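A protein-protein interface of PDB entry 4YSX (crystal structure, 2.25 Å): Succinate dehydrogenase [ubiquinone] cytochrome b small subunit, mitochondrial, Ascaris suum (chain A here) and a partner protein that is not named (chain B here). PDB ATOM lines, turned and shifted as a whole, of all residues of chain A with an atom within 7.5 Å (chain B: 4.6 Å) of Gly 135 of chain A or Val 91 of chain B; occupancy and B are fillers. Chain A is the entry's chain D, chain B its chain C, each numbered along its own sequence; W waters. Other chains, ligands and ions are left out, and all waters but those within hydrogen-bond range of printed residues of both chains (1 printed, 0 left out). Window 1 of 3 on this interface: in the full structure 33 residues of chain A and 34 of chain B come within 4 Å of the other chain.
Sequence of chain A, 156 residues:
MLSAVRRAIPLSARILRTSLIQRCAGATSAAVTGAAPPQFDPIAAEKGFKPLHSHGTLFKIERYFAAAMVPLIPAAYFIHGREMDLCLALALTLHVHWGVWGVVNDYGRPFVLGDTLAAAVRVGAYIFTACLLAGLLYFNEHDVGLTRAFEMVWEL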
ATOM      1  N   PHE A 128     -20.444   0.151 -29.736  1.00  0.00           N
ATOM      2  CA  PHE A 128     -19.115  -0.300 -29.302  1.00  0.00           C
ATOM      3  C   PHE A 128     -19.214  -1.246 -28.100  1.00  0.00           C
ATOM      4  O   PHE A 128     -18.589  -2.309 -28.081  1.00  0.00           O
ATOM      5  CB  PHE A 128     -18.233   0.896 -28.926  1.00  0.00           C
ATOM      6  CG  PHE A 128     -16.790   0.545 -28.677  1.00  0.00           C
ATOM      7  CD1 PHE A 128     -15.820   0.798 -29.649  1.00  0.00           C
ATOM      8  CD2 PHE A 128     -16.387  -0.003 -27.471  1.00  0.00           C
ATOM      9  CE1 PHE A 128     -14.484   0.495 -29.427  1.00  0.00           C
ATOM     10  CE2 PHE A 128     -15.046  -0.312 -27.240  1.00  0.00           C
ATOM     11  CZ  PHE A 128     -14.097  -0.066 -28.220  1.00  0.00           C
ATOM     12  N   THR A 129     -19.965  -0.831 -27.089  1.00  0.00           N
ATOM     13  CA  THR A 129     -20.077  -1.603 -25.863  1.00  0.00           C
ATOM     14  C   THR A 129     -20.711  -2.964 -26.205  1.00  0.00           C
ATOM     15  O   THR A 129     -20.118  -4.015 -25.963  1.00  0.00           O
ATOM     16  CB  THR A 129     -20.907  -0.846 -24.814  1.00  0.00           C
ATOM     17  OG1 THR A 129     -20.241   0.375 -24.452  1.00  0.00           O
ATOM     18  CG2 THR A 129     -21.124  -1.699 -23.552  1.00  0.00           C
ATOM     19  N   ALA A 130     -21.888  -2.920 -26.815  1.00  0.00           N
ATOM     20  CA  ALA A 130     -22.607  -4.115 -27.269  1.00  0.00           C
ATOM     21  C   ALA A 130     -21.734  -5.094 -28.028  1.00  0.00           C
ATOM     22  O   ALA A 130     -21.725  -6.281 -27.718  1.00  0.00           O
ATOM     23  CB  ALA A 130     -23.775  -3.703 -28.149  1.00  0.00           C
ATOM     24  N   CYS A 131     -21.002  -4.600 -29.027  1.00  0.00           N
ATOM     25  CA  CYS A 131     -20.155  -5.459 -29.834  1.00  0.00           C
ATOM     26  C   CYS A 131     -18.987  -5.997 -29.033  1.00  0.00           C
ATOM     27  O   CYS A 131     -18.521  -7.113 -29.293  1.00  0.00           O
ATOM     28  CB  CYS A 131     -19.628  -4.726 -31.078  1.00  0.00           C
ATOM     29  SG  CYS A 131     -20.898  -4.321 -32.302  1.00  0.00           S
ATOM     30  N   LEU A 132     -18.500  -5.198 -28.082  1.00  0.00           N
ATOM     31  CA  LEU A 132     -17.361  -5.590 -27.248  1.00  0.00           C
ATOM     32  C   LEU A 132     -17.715  -6.834 -26.438  1.00  0.00           C
ATOM     33  O   LEU A 132     -16.977  -7.823 -26.442  1.00  0.00           O
ATOM     34  CB  LEU A 132     -16.948  -4.449 -26.304  1.00  0.00           C
ATOM     35  CG  LEU A 132     -15.890  -4.778 -25.240  1.00  0.00           C
ATOM     36  CD1 LEU A 132     -14.579  -5.133 -25.900  1.00  0.00           C
ATOM     37  CD2 LEU A 132     -15.680  -3.634 -24.268  1.00  0.00           C
ATOM     38  N   LEU A 133     -18.852  -6.770 -25.752  1.00  0.00           N
ATOM     39  CA  LEU A 133     -19.311  -7.867 -24.918  1.00  0.00           C
ATOM     40  C   LEU A 133     -19.600  -9.105 -25.748  1.00  0.00           C
ATOM     41  O   LEU A 133     -19.209 -10.196 -25.369  1.00  0.00           O
ATOM     42  CB  LEU A 133     -20.561  -7.478 -24.158  1.00  0.00           C
ATOM     43  CG  LEU A 133     -21.120  -8.570 -23.247  1.00  0.00           C
ATOM     44  CD1 LEU A 133     -20.164  -8.891 -22.104  1.00  0.00           C
ATOM     45  CD2 LEU A 133     -22.489  -8.152 -22.722  1.00  0.00           C
ATOM     46  N   ALA A 134     -20.272  -8.929 -26.883  1.00  0.00           N
ATOM     47  CA  ALA A 134     -20.676 -10.061 -27.708  1.00  0.00           C
ATOM     48  C   ALA A 134     -19.453 -10.791 -28.206  1.00  0.00           C
ATOM     49  O   ALA A 134     -19.401 -12.025 -28.176  1.00  0.00           O
ATOM     50  CB  ALA A 134     -21.531  -9.605 -28.875  1.00  0.00           C
ATOM     51  N   GLY A 135     -18.463 -10.025 -28.660  1.00  0.00           N
ATOM     52  CA  GLY A 135     -17.212 -10.604 -29.142  1.00  0.00           C
ATOM     53  C   GLY A 135     -16.417 -11.265 -28.026  1.00  0.00           C
ATOM     54  O   GLY A 135     -15.731 -12.255 -28.246  1.00  0.00           O
ATOM     55  N   LEU A 136     -16.500 -10.710 -26.824  1.00  0.00           N
ATOM     56  CA  LEU A 136     -15.839 -11.325 -25.663  1.00  0.00           C
ATOM     57  C   LEU A 136     -16.521 -12.628 -25.266  1.00  0.00           C
ATOM     58  O   LEU A 136     -15.856 -13.636 -25.049  1.00  0.00           O
ATOM     59  CB  LEU A 136     -15.805 -10.362 -24.464  1.00  0.00           C
ATOM     60  CG  LEU A 136     -14.484  -9.614 -24.226  1.00  0.00           C
ATOM     61  CD1 LEU A 136     -13.716  -9.343 -25.516  1.00  0.00           C
ATOM     62  CD2 LEU A 136     -14.733  -8.323 -23.460  1.00  0.00           C
ATOM     63  N   LEU A 137     -17.842 -12.596 -25.149  1.00  0.00           N
ATOM     64  CA  LEU A 137     -18.598 -13.804 -24.856  1.00  0.00           C
ATOM     65  C   LEU A 137     -18.273 -14.871 -25.887  1.00  0.00           C
ATOM     66  O   LEU A 137     -17.986 -16.010 -25.524  1.00  0.00           O
ATOM     67  CB  LEU A 137     -20.104 -13.528 -24.812  1.00  0.00           C
ATOM     68  CG  LEU A 137     -20.586 -12.624 -23.678  1.00  0.00           C
ATOM     69  CD1 LEU A 137     -22.049 -12.288 -23.873  1.00  0.00           C
ATOM     70  CD2 LEU A 137     -20.355 -13.249 -22.307  1.00  0.00           C
ATOM     71  N   TYR A 138     -18.275 -14.500 -27.166  1.00  0.00           N
ATOM     72  CA  TYR A 138     -17.867 -15.429 -28.201  1.00  0.00           C
ATOM     73  C   TYR A 138     -16.501 -15.993 -27.866  1.00  0.00           C
ATOM     74  O   TYR A 138     -16.339 -17.195 -27.699  1.00  0.00           O
ATOM     75  CB  TYR A 138     -17.814 -14.790 -29.582  1.00  0.00           C
ATOM     76  CG  TYR A 138     -17.117 -15.697 -30.554  1.00  0.00           C
ATOM     77  CD1 TYR A 138     -15.735 -15.617 -30.743  1.00  0.00           C
ATOM     78  CD2 TYR A 138     -17.823 -16.679 -31.248  1.00  0.00           C
ATOM     79  CE1 TYR A 138     -15.080 -16.471 -31.609  1.00  0.00           C
ATOM     80  CE2 TYR A 138     -17.176 -17.541 -32.122  1.00  0.00           C
ATOM     81  CZ  TYR A 138     -15.804 -17.437 -32.290  1.00  0.00           C
ATOM     82  OH  TYR A 138     -15.142 -18.279 -33.157  1.00  0.00           O
ATOM     83  N   PHE A 139     -15.519 -15.114 -27.748  1.00  0.00           N
ATOM     84  CA  PHE A 139     -14.149 -15.535 -27.525  1.00  0.00           C
ATOM     85  C   PHE A 139     -14.025 -16.475 -26.321  1.00  0.00           C
ATOM     86  O   PHE A 139     -13.292 -17.467 -26.397  1.00  0.00           O
ATOM     87  CB  PHE A 139     -13.220 -14.321 -27.361  1.00  0.00           C
ATOM     88  CG  PHE A 139     -11.761 -14.676 -27.383  1.00  0.00           C
ATOM     89  CD1 PHE A 139     -11.113 -14.890 -28.583  1.00  0.00           C
ATOM     90  CD2 PHE A 139     -11.044 -14.806 -26.209  1.00  0.00           C
ATOM     91  CE1 PHE A 139      -9.768 -15.223 -28.625  1.00  0.00           C
ATOM     92  CE2 PHE A 139      -9.698 -15.134 -26.238  1.00  0.00           C
ATOM     93  CZ  PHE A 139      -9.062 -15.349 -27.448  1.00  0.00           C
ATOM     94  N   ASN A 140     -14.735 -16.161 -25.232  1.00  0.00           N
ATOM     95  CA  ASN A 140     -14.708 -16.976 -24.006  1.00  0.00           C
ATOM     96  C   ASN A 140     -15.433 -18.311 -24.180  1.00  0.00           C
ATOM     97  O   ASN A 140     -15.095 -19.285 -23.514  1.00  0.00           O
ATOM     98  CB  ASN A 140     -15.328 -16.230 -22.803  1.00  0.00           C
ATOM     99  CG  ASN A 140     -14.443 -15.106 -22.264  1.00  0.00           C
ATOM    100  OD1 ASN A 140     -14.885 -14.295 -21.451  1.00  0.00           O
ATOM    101  ND2 ASN A 140     -13.204 -15.058 -22.700  1.00  0.00           N
ATOM    102  N   GLU A 141     -16.417 -18.358 -25.079  1.00  0.00           N
ATOM    103  CA  GLU A 141     -17.269 -19.550 -25.238  1.00  0.00           C
ATOM    104  C   GLU A 141     -16.862 -20.502 -26.373  1.00  0.00           C
ATOM    105  O   GLU A 141     -17.171 -21.680 -26.304  1.00  0.00           O
ATOM    106  CB  GLU A 141     -18.728 -19.128 -25.399  1.00  0.00           C
ATOM    107  CG  GLU A 141     -19.283 -18.460 -24.145  1.00  0.00           C
ATOM    108  CD  GLU A 141     -20.504 -17.594 -24.394  1.00  0.00           C
ATOM    109  OE1 GLU A 141     -21.060 -17.099 -23.398  1.00  0.00           O
ATOM    110  OE2 GLU A 141     -20.913 -17.394 -25.565  1.00  0.00           O
ATOM    111  N   LEU B  87     -11.996  -5.406 -28.587  1.00  0.00           N
ATOM    112  CA  LEU B  87     -13.047  -5.393 -29.615  1.00  0.00           C
ATOM    113  C   LEU B  87     -12.611  -6.072 -30.900  1.00  0.00           C
ATOM    114  O   LEU B  87     -13.310  -6.959 -31.392  1.00  0.00           O
ATOM    115  CB  LEU B  87     -13.467  -3.969 -29.949  1.00  0.00           C
ATOM    116  CG  LEU B  87     -14.622  -3.789 -30.943  1.00  0.00           C
ATOM    117  CD1 LEU B  87     -15.927  -4.308 -30.355  1.00  0.00           C
ATOM    118  CD2 LEU B  87     -14.774  -2.320 -31.320  1.00  0.00           C
ATOM    119  N   ILE B  88     -11.484  -5.633 -31.462  1.00  0.00           N
ATOM    120  CA  ILE B  88     -10.978  -6.206 -32.718  1.00  0.00           C
ATOM    121  C   ILE B  88     -10.698  -7.696 -32.536  1.00  0.00           C
ATOM    122  O   ILE B  88     -11.009  -8.495 -33.409  1.00  0.00           O
ATOM    123  CB  ILE B  88      -9.692  -5.497 -33.235  1.00  0.00           C
ATOM    124  CG1 ILE B  88      -9.967  -4.023 -33.574  1.00  0.00           C
ATOM    125  CG2 ILE B  88      -9.130  -6.205 -34.465  1.00  0.00           C
ATOM    126  CD1 ILE B  88     -11.154  -3.806 -34.496  1.00  0.00           C
ATOM    127  N   GLY B  89     -10.123  -8.063 -31.393  1.00  0.00           N
ATOM    128  CA  GLY B  89      -9.850  -9.466 -31.078  1.00  0.00           C
ATOM    129  C   GLY B  89     -11.102 -10.321 -30.952  1.00  0.00           C
ATOM    130  O   GLY B  89     -11.249 -11.325 -31.644  1.00  0.00           O
ATOM    131  N   GLY B  90     -12.014  -9.914 -30.080  1.00  0.00           N
ATOM    132  CA  GLY B  90     -13.218 -10.697 -29.805  1.00  0.00           C
ATOM    133  C   GLY B  90     -14.105 -10.875 -31.020  1.00  0.00           C
ATOM    134  O   GLY B  90     -14.530 -11.983 -31.328  1.00  0.00           O
ATOM    135  N   VAL B  91     -14.366  -9.781 -31.723  1.00  0.00           N
ATOM    136  CA  VAL B  91     -15.222  -9.812 -32.899  1.00  0.00           C
ATOM    137  C   VAL B  91     -14.467 -10.373 -34.106  1.00  0.00           C
ATOM    138  O   VAL B  91     -15.021 -11.166 -34.870  1.00  0.00           O
ATOM    139  CB  VAL B  91     -15.808  -8.417 -33.201  1.00  0.00           C
ATOM    140  CG1 VAL B  91     -16.693  -8.449 -34.444  1.00  0.00           C
ATOM    141  CG2 VAL B  91     -16.593  -7.908 -31.998  1.00  0.00           C
ATOM    142  N   GLY B  92     -13.202  -9.990 -34.260  1.00  0.00           N
ATOM    143  CA  GLY B  92     -12.391 -10.452 -35.388  1.00  0.00           C
ATOM    144  C   GLY B  92     -12.301 -11.964 -35.466  1.00  0.00           C
ATOM    145  O   GLY B  92     -12.673 -12.564 -36.474  1.00  0.00           O
ATOM    146  N   PHE B  93     -11.827 -12.585 -34.393  1.00  0.00           N
ATOM    147  CA  PHE B  93     -11.726 -14.032 -34.352  1.00  0.00           C
ATOM    148  C   PHE B  93     -13.071 -14.718 -34.598  1.00  0.00           C
ATOM    149  O   PHE B  93     -13.126 -15.769 -35.233  1.00  0.00           O
ATOM    150  CB  PHE B  93     -11.094 -14.497 -33.035  1.00  0.00           C
ATOM    151  CG  PHE B  93      -9.602 -14.312 -32.995  1.00  0.00           C
ATOM    152  CD1 PHE B  93      -9.017 -13.359 -32.173  1.00  0.00           C
ATOM    153  CD2 PHE B  93      -8.780 -15.076 -33.808  1.00  0.00           C
ATOM    154  CE1 PHE B  93      -7.643 -13.185 -32.153  1.00  0.00           C
ATOM    155  CE2 PHE B  93      -7.407 -14.907 -33.793  1.00  0.00           C
ATOM    156  CZ  PHE B  93      -6.838 -13.957 -32.967  1.00  0.00           C
ATOM    157  N   SER B  94     -14.154 -14.115 -34.123  1.00  0.00           N
ATOM    158  CA  SER B  94     -15.483 -14.672 -34.344  1.00  0.00           C
ATOM    159  C   SER B  94     -15.871 -14.615 -35.820  1.00  0.00           C
ATOM    160  O   SER B  94     -16.381 -15.588 -36.365  1.00  0.00           O
ATOM    161  CB  SER B  94     -16.531 -13.956 -33.477  1.00  0.00           C
ATOM    162  OG  SER B  94     -16.962 -12.742 -34.061  1.00  0.00           O
ATOM    163  N   VAL B  95     -15.611 -13.481 -36.464  1.00  0.00           N
ATOM    164  CA  VAL B  95     -15.985 -13.286 -37.867  1.00  0.00           C
ATOM    165  C   VAL B  95     -15.034 -14.022 -38.823  1.00  0.00           C
ATOM    166  O   VAL B  95     -15.427 -14.343 -39.940  1.00  0.00           O
ATOM    167  CB  VAL B  95     -16.085 -11.775 -38.217  1.00  0.00           C
ATOM    168  CG1 VAL B  95     -16.341 -11.554 -39.703  1.00  0.00           C
ATOM    169  CG2 VAL B  95     -17.203 -11.128 -37.416  1.00  0.00           C
HETATM  170  O   HOH W   1     -12.279 -18.115 -33.030  1.00  0.00           O
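Water W1 bridges OH of Tyr 138 of chain A and O of Phe 93 of chain B.
Of chain B, only Gly 90 (3.3 Å) and Val 91 (3.9 Å) come within 4 Å of Gly 135 of chain A.
Val 91 of chain B touches just these residues of chain A: Cys 131 (3.4 Å) and Gly 135 (3.9 Å).
Of chain A, only Gly 135 (3.3 Å) and Tyr 138 (3.9 Å) come within 4 Å of Gly 90 of chain B.
Printed residues of chain B within 4 Å of Leu 132 of chain A: Leu 87.
Of the printed residues of chain A, Leu 87 of chain B touches Phe 128, Cys 131 and Leu 132.
Of the printed residues of chain B, Tyr 138 of chain A touches Gly 90, Phe 93 and Ser 94.
Printed residues of chain B within 4 Å of Phe 128 of chain A: Leu 87.
Printed residues of chain A within 4 Å of Phe 93 of chain B: Tyr 138.
Leu 136 of chain A touches none of the printed residues of chain B.
Ala 130 of chain A touches none of the printed residues of chain B.
The nearest residue of chain A that does not touch Val 91 of chain B is Leu 132 of chain A (5.1 Å).
Of the 14 printed residues of chain A, 5 touch a printed residue of chain B.
Printed residues of chain A that touch a printed residue of chain B: Phe 128, Cys 131, Leu 132, Gly 135 and Tyr 138.
Of the 9 printed residues of chain B, 5 touch a printed residue of chain A.
Along chain B the printed residues that touch a printed residue of chain A span positions 87 to 94.
Among the printed residues, 9 pairs touch across the chains.
Among the printed residues, no Asp or Glu carboxylate lies within 4 Å of a Lys or Arg side-chain nitrogen of the other chain.
The backbone carbonyl oxygen (O) of Val 91 of chain B is in hydrogen-bond range of the side-chain hydroxyl (OG) of Ser 94 of chain B, 2.6 Å away.
The backbone carbonyl oxygen (O) of Gly 90 of chain B lies close to the backbone carbonyl oxygen (O) of Gly 135 of chain A, 3.3 Å away.
Among the printed residues, pairs that only touch across the chains: Phe 128 of chain A with Leu 87 of chain B (3.4 Å), Cys 131 of chain A with Leu 87 of chain B (3.7 Å), Cys 131 of chain A with Val 91 of chain B (3.4 Å), Leu 132 of chain A with Leu 87 of chain B (3.5 Å), Gly 135 of chain A with Val 91 of chain B (3.9 Å), Tyr 138 of chain A with Gly 90 of chain B (3.9 Å), Tyr 138 of chain A with Phe 93 of chain B (3.8 Å) and Tyr 138 of chain A with Ser 94 of chain B (3.3 Å).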
